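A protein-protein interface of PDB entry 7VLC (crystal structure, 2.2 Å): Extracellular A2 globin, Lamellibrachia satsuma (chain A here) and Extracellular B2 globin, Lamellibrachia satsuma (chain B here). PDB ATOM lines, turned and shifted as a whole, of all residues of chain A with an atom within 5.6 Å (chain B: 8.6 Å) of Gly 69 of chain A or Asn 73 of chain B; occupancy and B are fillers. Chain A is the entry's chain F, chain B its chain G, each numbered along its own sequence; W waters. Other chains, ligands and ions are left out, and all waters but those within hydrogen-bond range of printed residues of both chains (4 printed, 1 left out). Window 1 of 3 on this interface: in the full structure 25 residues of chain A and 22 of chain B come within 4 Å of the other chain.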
ATOM      1  N   TYR A  19     -16.145  28.560  21.364  1.00  0.00           N
ATOM      2  CA  TYR A  19     -15.394  28.063  20.214  1.00  0.00           C
ATOM      3  C   TYR A  19     -16.318  27.387  19.208  1.00  0.00           C
ATOM      4  O   TYR A  19     -16.133  27.527  17.994  1.00  0.00           O
ATOM      5  CB  TYR A  19     -14.309  27.098  20.695  1.00  0.00           C
ATOM      6  CG  TYR A  19     -13.242  26.750  19.683  1.00  0.00           C
ATOM      7  CD1 TYR A  19     -12.688  27.722  18.859  1.00  0.00           C
ATOM      8  CD2 TYR A  19     -12.754  25.453  19.587  1.00  0.00           C
ATOM      9  CE1 TYR A  19     -11.693  27.402  17.942  1.00  0.00           C
ATOM     10  CE2 TYR A  19     -11.760  25.123  18.682  1.00  0.00           C
ATOM     11  CZ  TYR A  19     -11.232  26.097  17.860  1.00  0.00           C
ATOM     12  OH  TYR A  19     -10.245  25.754  16.958  1.00  0.00           O
ATOM     13  N   ALA A  64      -4.750  33.168  13.338  1.00  0.00           N
ATOM     14  CA  ALA A  64      -5.741  33.097  14.409  1.00  0.00           C
ATOM     15  C   ALA A  64      -6.324  31.694  14.535  1.00  0.00           C
ATOM     16  O   ALA A  64      -6.621  31.242  15.646  1.00  0.00           O
ATOM     17  CB  ALA A  64      -6.855  34.118  14.167  1.00  0.00           C
ATOM     18  N   THR A  65      -6.507  30.999  13.410  1.00  0.00           N
ATOM     19  CA  THR A  65      -6.952  29.609  13.465  1.00  0.00           C
ATOM     20  C   THR A  65      -5.970  28.748  14.256  1.00  0.00           C
ATOM     21  O   THR A  65      -6.381  27.912  15.069  1.00  0.00           O
ATOM     22  CB  THR A  65      -7.131  29.063  12.048  1.00  0.00           C
ATOM     23  OG1 THR A  65      -8.187  29.777  11.396  1.00  0.00           O
ATOM     24  CG2 THR A  65      -7.466  27.578  12.072  1.00  0.00           C
ATOM     25  N   ARG A  66      -4.667  28.957  14.050  1.00  0.00           N
ATOM     26  CA  ARG A  66      -3.678  28.168  14.780  1.00  0.00           C
ATOM     27  C   ARG A  66      -3.668  28.526  16.262  1.00  0.00           C
ATOM     28  O   ARG A  66      -3.543  27.642  17.117  1.00  0.00           O
ATOM     29  CB  ARG A  66      -2.287  28.366  14.169  1.00  0.00           C
ATOM     30  CG  ARG A  66      -2.166  27.909  12.717  1.00  0.00           C
ATOM     31  CD  ARG A  66      -0.720  27.945  12.210  1.00  0.00           C
ATOM     32  NE  ARG A  66      -0.281  29.296  11.881  1.00  0.00           N
ATOM     33  CZ  ARG A  66      -0.454  29.868  10.693  1.00  0.00           C
ATOM     34  NH1 ARG A  66      -0.027  31.106  10.479  1.00  0.00           N
ATOM     35  NH2 ARG A  66      -1.054  29.202   9.717  1.00  0.00           N
ATOM     36  N   VAL A  67      -3.808  29.813  16.585  1.00  0.00           N
ATOM     37  CA  VAL A  67      -3.792  30.242  17.981  1.00  0.00           C
ATOM     38  C   VAL A  67      -4.967  29.635  18.743  1.00  0.00           C
ATOM     39  O   VAL A  67      -4.797  29.053  19.821  1.00  0.00           O
ATOM     40  CB  VAL A  67      -3.804  31.777  18.069  1.00  0.00           C
ATOM     41  CG1 VAL A  67      -3.842  32.208  19.514  1.00  0.00           C
ATOM     42  CG2 VAL A  67      -2.594  32.357  17.368  1.00  0.00           C
ATOM     43  N   LEU A  68      -6.184  29.781  18.200  1.00  0.00           N
ATOM     44  CA  LEU A  68      -7.360  29.233  18.874  1.00  0.00           C
ATOM     45  C   LEU A  68      -7.285  27.714  18.962  1.00  0.00           C
ATOM     46  O   LEU A  68      -7.720  27.121  19.956  1.00  0.00           O
ATOM     47  CB  LEU A  68      -8.636  29.661  18.153  1.00  0.00           C
ATOM     48  CG  LEU A  68      -8.888  31.163  17.978  1.00  0.00           C
ATOM     49  CD1 LEU A  68     -10.354  31.420  17.668  1.00  0.00           C
ATOM     50  CD2 LEU A  68      -8.440  31.962  19.188  1.00  0.00           C
ATOM     51  N   GLY A  69      -6.735  27.068  17.929  1.00  0.00           N
ATOM     52  CA  GLY A  69      -6.518  25.632  18.001  1.00  0.00           C
ATOM     53  C   GLY A  69      -5.541  25.254  19.097  1.00  0.00           C
ATOM     54  O   GLY A  69      -5.689  24.213  19.746  1.00  0.00           O
ATOM     55  N   GLY A  70      -4.527  26.095  19.318  1.00  0.00           N
ATOM     56  CA  GLY A  70      -3.627  25.871  20.435  1.00  0.00           C
ATOM     57  C   GLY A  70      -4.324  26.022  21.772  1.00  0.00           C
ATOM     58  O   GLY A  70      -4.106  25.224  22.686  1.00  0.00           O
ATOM     59  N   LEU A  71      -5.176  27.045  21.906  1.00  0.00           N
ATOM     60  CA  LEU A  71      -5.975  27.183  23.119  1.00  0.00           C
ATOM     61  C   LEU A  71      -6.907  25.993  23.300  1.00  0.00           C
ATOM     62  O   LEU A  71      -7.063  25.480  24.412  1.00  0.00           O
ATOM     63  CB  LEU A  71      -6.786  28.478  23.078  1.00  0.00           C
ATOM     64  CG  LEU A  71      -6.097  29.761  23.525  1.00  0.00           C
ATOM     65  CD1 LEU A  71      -6.996  30.949  23.241  1.00  0.00           C
ATOM     66  CD2 LEU A  71      -5.764  29.680  25.002  1.00  0.00           C
ATOM     67  N   ASP A  72      -7.547  25.548  22.217  1.00  0.00           N
ATOM     68  CA  ASP A  72      -8.481  24.435  22.319  1.00  0.00           C
ATOM     69  C   ASP A  72      -7.787  23.186  22.843  1.00  0.00           C
ATOM     70  O   ASP A  72      -8.339  22.465  23.685  1.00  0.00           O
ATOM     71  CB  ASP A  72      -9.117  24.170  20.959  1.00  0.00           C
ATOM     72  CG  ASP A  72     -10.127  23.043  21.001  1.00  0.00           C
ATOM     73  OD1 ASP A  72     -11.277  23.303  21.402  1.00  0.00           O
ATOM     74  OD2 ASP A  72      -9.771  21.903  20.633  1.00  0.00           O
ATOM     75  N   MET A  73      -6.567  22.917  22.360  1.00  0.00           N
ATOM     76  CA  MET A  73      -5.825  21.750  22.825  1.00  0.00           C
ATOM     77  C   MET A  73      -5.545  21.841  24.318  1.00  0.00           C
ATOM     78  O   MET A  73      -5.686  20.852  25.044  1.00  0.00           O
ATOM     79  CB  MET A  73      -4.524  21.596  22.031  1.00  0.00           C
ATOM     80  CG  MET A  73      -4.717  21.107  20.588  1.00  0.00           C
ATOM     81  SD  MET A  73      -3.183  20.732  19.705  1.00  0.00           S
ATOM     82  CE  MET A  73      -2.464  22.369  19.614  1.00  0.00           C
ATOM     83  N   CYS A  74      -5.175  23.028  24.801  1.00  0.00           N
ATOM     84  CA  CYS A  74      -4.912  23.185  26.227  1.00  0.00           C
ATOM     85  C   CYS A  74      -6.184  23.007  27.044  1.00  0.00           C
ATOM     86  O   CYS A  74      -6.170  22.336  28.083  1.00  0.00           O
ATOM     87  CB  CYS A  74      -4.291  24.553  26.507  1.00  0.00           C
ATOM     88  SG  CYS A  74      -2.677  24.811  25.752  1.00  0.00           S
ATOM     89  N   TRP B  17     -17.187  14.788  10.555  1.00  0.00           N
ATOM     90  CA  TRP B  17     -16.181  15.166  11.538  1.00  0.00           C
ATOM     91  C   TRP B  17     -16.814  15.722  12.808  1.00  0.00           C
ATOM     92  O   TRP B  17     -16.344  15.430  13.913  1.00  0.00           O
ATOM     93  CB  TRP B  17     -15.220  16.187  10.927  1.00  0.00           C
ATOM     94  CG  TRP B  17     -14.016  16.451  11.755  1.00  0.00           C
ATOM     95  CD1 TRP B  17     -13.689  17.615  12.384  1.00  0.00           C
ATOM     96  CD2 TRP B  17     -12.965  15.526  12.048  1.00  0.00           C
ATOM     97  NE1 TRP B  17     -12.498  17.473  13.051  1.00  0.00           N
ATOM     98  CE2 TRP B  17     -12.032  16.198  12.860  1.00  0.00           C
ATOM     99  CE3 TRP B  17     -12.723  14.192  11.702  1.00  0.00           C
ATOM    100  CZ2 TRP B  17     -10.874  15.582  13.332  1.00  0.00           C
ATOM    101  CZ3 TRP B  17     -11.575  13.583  12.172  1.00  0.00           C
ATOM    102  CH2 TRP B  17     -10.666  14.277  12.977  1.00  0.00           C
ATOM    103  N   TRP B  21     -16.189  14.517  16.700  1.00  0.00           N
ATOM    104  CA  TRP B  21     -15.247  15.362  17.429  1.00  0.00           C
ATOM    105  C   TRP B  21     -15.781  15.721  18.812  1.00  0.00           C
ATOM    106  O   TRP B  21     -16.929  16.150  18.960  1.00  0.00           O
ATOM    107  CB  TRP B  21     -14.965  16.622  16.613  1.00  0.00           C
ATOM    108  CG  TRP B  21     -14.385  17.782  17.368  1.00  0.00           C
ATOM    109  CD1 TRP B  21     -15.064  18.684  18.137  1.00  0.00           C
ATOM    110  CD2 TRP B  21     -13.013  18.202  17.379  1.00  0.00           C
ATOM    111  NE1 TRP B  21     -14.199  19.621  18.646  1.00  0.00           N
ATOM    112  CE2 TRP B  21     -12.935  19.349  18.195  1.00  0.00           C
ATOM    113  CE3 TRP B  21     -11.844  17.713  16.787  1.00  0.00           C
ATOM    114  CZ2 TRP B  21     -11.736  20.015  18.433  1.00  0.00           C
ATOM    115  CZ3 TRP B  21     -10.652  18.375  17.029  1.00  0.00           C
ATOM    116  CH2 TRP B  21     -10.607  19.512  17.843  1.00  0.00           C
ATOM    117  N   ARG B  29     -10.798  12.362  20.812  1.00  0.00           N
ATOM    118  CA  ARG B  29      -9.805  12.729  19.810  1.00  0.00           C
ATOM    119  C   ARG B  29      -8.607  11.791  19.857  1.00  0.00           C
ATOM    120  O   ARG B  29      -8.056  11.422  18.814  1.00  0.00           O
ATOM    121  CB  ARG B  29      -9.344  14.169  20.029  1.00  0.00           C
ATOM    122  CG  ARG B  29     -10.443  15.160  20.345  1.00  0.00           C
ATOM    123  CD  ARG B  29      -9.834  16.530  20.590  1.00  0.00           C
ATOM    124  NE  ARG B  29     -10.811  17.528  21.012  1.00  0.00           N
ATOM    125  CZ  ARG B  29     -10.505  18.794  21.269  1.00  0.00           C
ATOM    126  NH1 ARG B  29      -9.251  19.206  21.142  1.00  0.00           N
ATOM    127  NH2 ARG B  29     -11.448  19.647  21.650  1.00  0.00           N
ATOM    128  N   ALA B  33      -6.968   9.297  16.663  1.00  0.00           N
ATOM    129  CA  ALA B  33      -5.620   9.497  16.144  1.00  0.00           C
ATOM    130  C   ALA B  33      -4.726   8.292  16.434  1.00  0.00           C
ATOM    131  O   ALA B  33      -3.956   7.865  15.565  1.00  0.00           O
ATOM    132  CB  ALA B  33      -5.024  10.775  16.730  1.00  0.00           C
ATOM    133  N   ALA B  66       0.444  13.814  22.802  1.00  0.00           N
ATOM    134  CA  ALA B  66       0.414  15.222  22.425  1.00  0.00           C
ATOM    135  C   ALA B  66       0.503  15.391  20.913  1.00  0.00           C
ATOM    136  O   ALA B  66      -0.185  16.242  20.336  1.00  0.00           O
ATOM    137  CB  ALA B  66       1.547  15.976  23.122  1.00  0.00           C
ATOM    138  N   HIS B  67       1.335  14.582  20.252  1.00  0.00           N
ATOM    139  CA  HIS B  67       1.402  14.642  18.793  1.00  0.00           C
ATOM    140  C   HIS B  67       0.070  14.250  18.167  1.00  0.00           C
ATOM    141  O   HIS B  67      -0.403  14.910  17.234  1.00  0.00           O
ATOM    142  CB  HIS B  67       2.522  13.742  18.268  1.00  0.00           C
ATOM    143  CG  HIS B  67       2.579  13.666  16.773  1.00  0.00           C
ATOM    144  ND1 HIS B  67       3.050  14.700  15.993  1.00  0.00           N
ATOM    145  CD2 HIS B  67       2.203  12.689  15.915  1.00  0.00           C
ATOM    146  CE1 HIS B  67       2.970  14.361  14.719  1.00  0.00           C
ATOM    147  NE2 HIS B  67       2.460  13.146  14.644  1.00  0.00           N
ATOM    148  N   CYS B  68      -0.545  13.173  18.664  1.00  0.00           N
ATOM    149  CA  CYS B  68      -1.857  12.765  18.171  1.00  0.00           C
ATOM    150  C   CYS B  68      -2.875  13.892  18.307  1.00  0.00           C
ATOM    151  O   CYS B  68      -3.679  14.131  17.397  1.00  0.00           O
ATOM    152  CB  CYS B  68      -2.333  11.522  18.924  1.00  0.00           C
ATOM    153  SG  CYS B  68      -1.574   9.977  18.378  1.00  0.00           S
ATOM    154  N   ILE B  69      -2.845  14.605  19.431  1.00  0.00           N
ATOM    155  CA  ILE B  69      -3.768  15.716  19.631  1.00  0.00           C
ATOM    156  C   ILE B  69      -3.431  16.864  18.686  1.00  0.00           C
ATOM    157  O   ILE B  69      -4.328  17.525  18.146  1.00  0.00           O
ATOM    158  CB  ILE B  69      -3.753  16.145  21.108  1.00  0.00           C
ATOM    159  CG1 ILE B  69      -4.413  15.055  21.957  1.00  0.00           C
ATOM    160  CG2 ILE B  69      -4.440  17.489  21.300  1.00  0.00           C
ATOM    161  CD1 ILE B  69      -4.289  15.273  23.438  1.00  0.00           C
ATOM    162  N   ARG B  70      -2.140  17.101  18.443  1.00  0.00           N
ATOM    163  CA  ARG B  70      -1.756  18.133  17.486  1.00  0.00           C
ATOM    164  C   ARG B  70      -2.185  17.779  16.068  1.00  0.00           C
ATOM    165  O   ARG B  70      -2.568  18.670  15.301  1.00  0.00           O
ATOM    166  CB  ARG B  70      -0.245  18.373  17.542  1.00  0.00           C
ATOM    167  CG  ARG B  70       0.212  19.152  18.766  1.00  0.00           C
ATOM    168  CD  ARG B  70       1.656  19.623  18.624  1.00  0.00           C
ATOM    169  NE  ARG B  70       2.619  18.523  18.560  1.00  0.00           N
ATOM    170  CZ  ARG B  70       3.188  17.962  19.624  1.00  0.00           C
ATOM    171  NH1 ARG B  70       2.885  18.388  20.843  1.00  0.00           N
ATOM    172  NH2 ARG B  70       4.059  16.972  19.470  1.00  0.00           N
ATOM    173  N   VAL B  71      -2.150  16.495  15.709  1.00  0.00           N
ATOM    174  CA  VAL B  71      -2.517  16.089  14.355  1.00  0.00           C
ATOM    175  C   VAL B  71      -4.007  16.307  14.114  1.00  0.00           C
ATOM    176  O   VAL B  71      -4.405  16.944  13.131  1.00  0.00           O
ATOM    177  CB  VAL B  71      -2.112  14.625  14.097  1.00  0.00           C
ATOM    178  CG1 VAL B  71      -2.662  14.142  12.765  1.00  0.00           C
ATOM    179  CG2 VAL B  71      -0.601  14.477  14.116  1.00  0.00           C
ATOM    180  N   VAL B  72      -4.857  15.772  14.997  1.00  0.00           N
ATOM    181  CA  VAL B  72      -6.296  15.934  14.796  1.00  0.00           C
ATOM    182  C   VAL B  72      -6.682  17.404  14.847  1.00  0.00           C
ATOM    183  O   VAL B  72      -7.594  17.836  14.134  1.00  0.00           O
ATOM    184  CB  VAL B  72      -7.096  15.099  15.818  1.00  0.00           C
ATOM    185  CG1 VAL B  72      -6.911  13.618  15.548  1.00  0.00           C
ATOM    186  CG2 VAL B  72      -6.682  15.440  17.233  1.00  0.00           C
ATOM    187  N   ASN B  73      -5.989  18.201  15.668  1.00  0.00           N
ATOM    188  CA  ASN B  73      -6.227  19.641  15.676  1.00  0.00           C
ATOM    189  C   ASN B  73      -5.883  20.255  14.326  1.00  0.00           C
ATOM    190  O   ASN B  73      -6.576  21.161  13.849  1.00  0.00           O
ATOM    191  CB  ASN B  73      -5.417  20.305  16.791  1.00  0.00           C
ATOM    192  CG  ASN B  73      -5.593  21.814  16.823  1.00  0.00           C
ATOM    193  OD1 ASN B  73      -6.611  22.320  17.293  1.00  0.00           O
ATOM    194  ND2 ASN B  73      -4.594  22.542  16.326  1.00  0.00           N
ATOM    195  N   GLY B  74      -4.816  19.766  13.689  1.00  0.00           N
ATOM    196  CA  GLY B  74      -4.475  20.249  12.363  1.00  0.00           C
ATOM    197  C   GLY B  74      -5.487  19.832  11.314  1.00  0.00           C
ATOM    198  O   GLY B  74      -5.814  20.607  10.412  1.00  0.00           O
ATOM    199  N   LEU B  75      -5.999  18.605  11.421  1.00  0.00           N
ATOM    200  CA  LEU B  75      -7.028  18.155  10.489  1.00  0.00           C
ATOM    201  C   LEU B  75      -8.349  18.875  10.734  1.00  0.00           C
ATOM    202  O   LEU B  75      -9.063  19.216   9.783  1.00  0.00           O
ATOM    203  CB  LEU B  75      -7.210  16.642  10.600  1.00  0.00           C
ATOM    204  CG  LEU B  75      -8.272  16.039   9.683  1.00  0.00           C
ATOM    205  CD1 LEU B  75      -7.938  16.323   8.222  1.00  0.00           C
ATOM    206  CD2 LEU B  75      -8.408  14.546   9.938  1.00  0.00           C
ATOM    207  N   ASP B  76      -8.690  19.116  12.003  1.00  0.00           N
ATOM    208  CA  ASP B  76      -9.911  19.852  12.319  1.00  0.00           C
ATOM    209  C   ASP B  76      -9.838  21.287  11.815  1.00  0.00           C
ATOM    210  O   ASP B  76     -10.832  21.827  11.315  1.00  0.00           O
ATOM    211  CB  ASP B  76     -10.162  19.828  13.826  1.00  0.00           C
ATOM    212  CG  ASP B  76     -11.408  20.595  14.220  1.00  0.00           C
ATOM    213  OD1 ASP B  76     -12.517  20.084  13.984  1.00  0.00           O
ATOM    214  OD2 ASP B  76     -11.276  21.714  14.761  1.00  0.00           O
ATOM    215  N   SER B  77      -8.671  21.924  11.946  1.00  0.00           N
ATOM    216  CA  SER B  77      -8.504  23.265  11.396  1.00  0.00           C
ATOM    217  C   SER B  77      -8.691  23.255   9.888  1.00  0.00           C
ATOM    218  O   SER B  77      -9.283  24.181   9.321  1.00  0.00           O
ATOM    219  CB  SER B  77      -7.126  23.819  11.761  1.00  0.00           C
ATOM    220  OG  SER B  77      -6.114  23.241  10.950  1.00  0.00           O
ATOM    221  N   ALA B  78      -8.209  22.202   9.225  1.00  0.00           N
ATOM    222  CA  ALA B  78      -8.340  22.113   7.777  1.00  0.00           C
ATOM    223  C   ALA B  78      -9.775  21.815   7.372  1.00  0.00           C
ATOM    224  O   ALA B  78     -10.297  22.417   6.425  1.00  0.00           O
ATOM    225  CB  ALA B  78      -7.386  21.051   7.229  1.00  0.00           C
ATOM    226  N   ILE B  79     -10.435  20.901   8.083  1.00  0.00           N
ATOM    227  CA  ILE B  79     -11.827  20.591   7.770  1.00  0.00           C
ATOM    228  C   ILE B  79     -12.709  21.810   8.010  1.00  0.00           C
ATOM    229  O   ILE B  79     -13.597  22.121   7.207  1.00  0.00           O
ATOM    230  CB  ILE B  79     -12.300  19.375   8.586  1.00  0.00           C
ATOM    231  CG1 ILE B  79     -11.588  18.106   8.102  1.00  0.00           C
ATOM    232  CG2 ILE B  79     -13.815  19.227   8.502  1.00  0.00           C
ATOM    233  CD1 ILE B  79     -11.979  16.853   8.869  1.00  0.00           C
ATOM    234  N   GLY B  80     -12.464  22.531   9.105  1.00  0.00           N
ATOM    235  CA  GLY B  80     -13.245  23.723   9.388  1.00  0.00           C
ATOM    236  C   GLY B  80     -13.042  24.829   8.371  1.00  0.00           C
ATOM    237  O   GLY B  80     -13.970  25.590   8.087  1.00  0.00           O
ATOM    238  N   GLN B  91      -3.454  28.056   5.657  1.00  0.00           N
ATOM    239  CA  GLN B  91      -3.213  27.073   6.708  1.00  0.00           C
ATOM    240  C   GLN B  91      -2.498  25.846   6.160  1.00  0.00           C
ATOM    241  O   GLN B  91      -1.602  25.299   6.814  1.00  0.00           O
ATOM    242  CB  GLN B  91      -4.532  26.671   7.365  1.00  0.00           C
ATOM    243  CG  GLN B  91      -4.410  25.548   8.381  1.00  0.00           C
ATOM    244  CD  GLN B  91      -3.758  25.990   9.675  1.00  0.00           C
ATOM    245  OE1 GLN B  91      -3.438  27.167   9.857  1.00  0.00           O
ATOM    246  NE2 GLN B  91      -3.564  25.046  10.589  1.00  0.00           N
ATOM    247  N   LEU B  95       1.079  24.108   7.261  1.00  0.00           N
ATOM    248  CA  LEU B  95       1.162  22.678   7.540  1.00  0.00           C
ATOM    249  C   LEU B  95       2.174  21.992   6.634  1.00  0.00           C
ATOM    250  O   LEU B  95       2.848  21.048   7.063  1.00  0.00           O
ATOM    251  CB  LEU B  95      -0.209  22.021   7.383  1.00  0.00           C
ATOM    252  CG  LEU B  95      -1.219  22.208   8.519  1.00  0.00           C
ATOM    253  CD1 LEU B  95      -2.535  21.540   8.169  1.00  0.00           C
ATOM    254  CD2 LEU B  95      -0.670  21.658   9.829  1.00  0.00           C
HETATM  255  O   HOH W   1     -13.689  22.242  20.769  1.00  0.00           O
HETATM  256  O   HOH W   2     -11.452  21.920  23.953  1.00  0.00           O
HETATM  257  O   HOH W   3      -2.725  25.269  16.289  1.00  0.00           O
HETATM  258  O   HOH W   4      -9.541  23.092  17.253  1.00  0.00           O
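OG of Ser 77 of chain B lies within hydrogen-bond range of O of Gly 74 of chain B (2.7 Å).
The side-chain amide nitrogen of Gln 91 of chain B sits at hydrogen-bond distance from the side-chain hydroxyl of Ser 77 of chain B (3.1 Å).
Among the printed residues, pairs that only touch across the chains: Asp 72 of chain A with Trp 21 of chain B, Met 73 of chain A with Asn 73 of chain B, Met 73 of chain A with Arg 70 of chain B and Thr 65 of chain A with Ser 77 of chain B.
The guanidinium group (NH2) of Arg 66 of chain A is in hydrogen-bond range of the side-chain amide oxygen (OE1) of Gln 91 of chain B (3.1 Å).
The backbone carbonyl oxygen (O) of Gly 69 of chain A sits close to the side-chain amide oxygen (OD1) of Asn 73 of chain B, at 3.2 Å.
The guanidinium group (NH1) of Arg 29 of chain B lies within salt-bridge range of the side-chain carboxylate (OD2) of Asp 72 of chain A.
O of Ile 69 of chain B sits close to SD of Met 73 of chain A (3.7 Å).
Hydrophobic or aromatic side chains of chain B within 4 Å of the printed part of chain A: Trp 21 and Ile 69.
Of the 12 printed residues of chain A, 5 touch a printed residue of chain B.
Printed residues of chain A that touch a printed residue of chain B: Thr 65, Arg 66, Gly 69, Asp 72 and Met 73.
Hydrophobic or aromatic side chains of chain A within 4 Å of the printed part of chain B: Met 73.
Among the printed residues, 8 pairs touch across the chains.
Among the printed residues, Asp or Glu carboxylates within 4 Å of a Lys or Arg side-chain nitrogen of the other chain: Asp 72 of chain A with Arg 29 of chain B (2.8 Å).
Printed residues of chain B within 4 Å of Arg 66 of chain A: Gln 91.
Gly 69 of chain A touches one residue of chain B.
Printed residues of chain B within 4 Å of Met 73 of chain A: Ile 69, Arg 70 and Asn 73.
Of the printed residues of chain A, Trp 21 of chain B touches Asp 72.
Of the printed residues of chain A, Arg 29 of chain B touches Asp 72 (2.8 Å).
Of the printed residues of chain A, Arg 70 of chain B touches Met 73.
Of the printed residues of chain A, Asn 73 of chain B touches Gly 69 (3.2 Å) and Met 73 (3.7 Å).
The nearest printed residue of chain A that does not touch Asn 73 of chain B is Asp 72 of chain A (4.6 Å).
Water W3 lies within hydrogen-bond range of the backbone carbonyl oxygen of Arg 66 of chain A (2.6 Å) and the side-chain amide nitrogen of Asn 73 of chain B (3.3 Å).
Water W1 lies within hydrogen-bond range of the side-chain carboxylate (OD1) of Asp 72 of chain A (2.7 Å) and the indole nitrogen (NE1) of Trp 21 of chain B (3.4 Å).
Water W4 lies within hydrogen-bond range of the side-chain hydroxyl of Tyr 19 of chain A, the side-chain amide oxygen of Asn 73 of chain B and the side-chain carboxylate of Asp 76 of chain B.
Water W2 lies within hydrogen-bond range of OD1 of Asp 72 of chain A and NH2 of Arg 29 of chain B.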
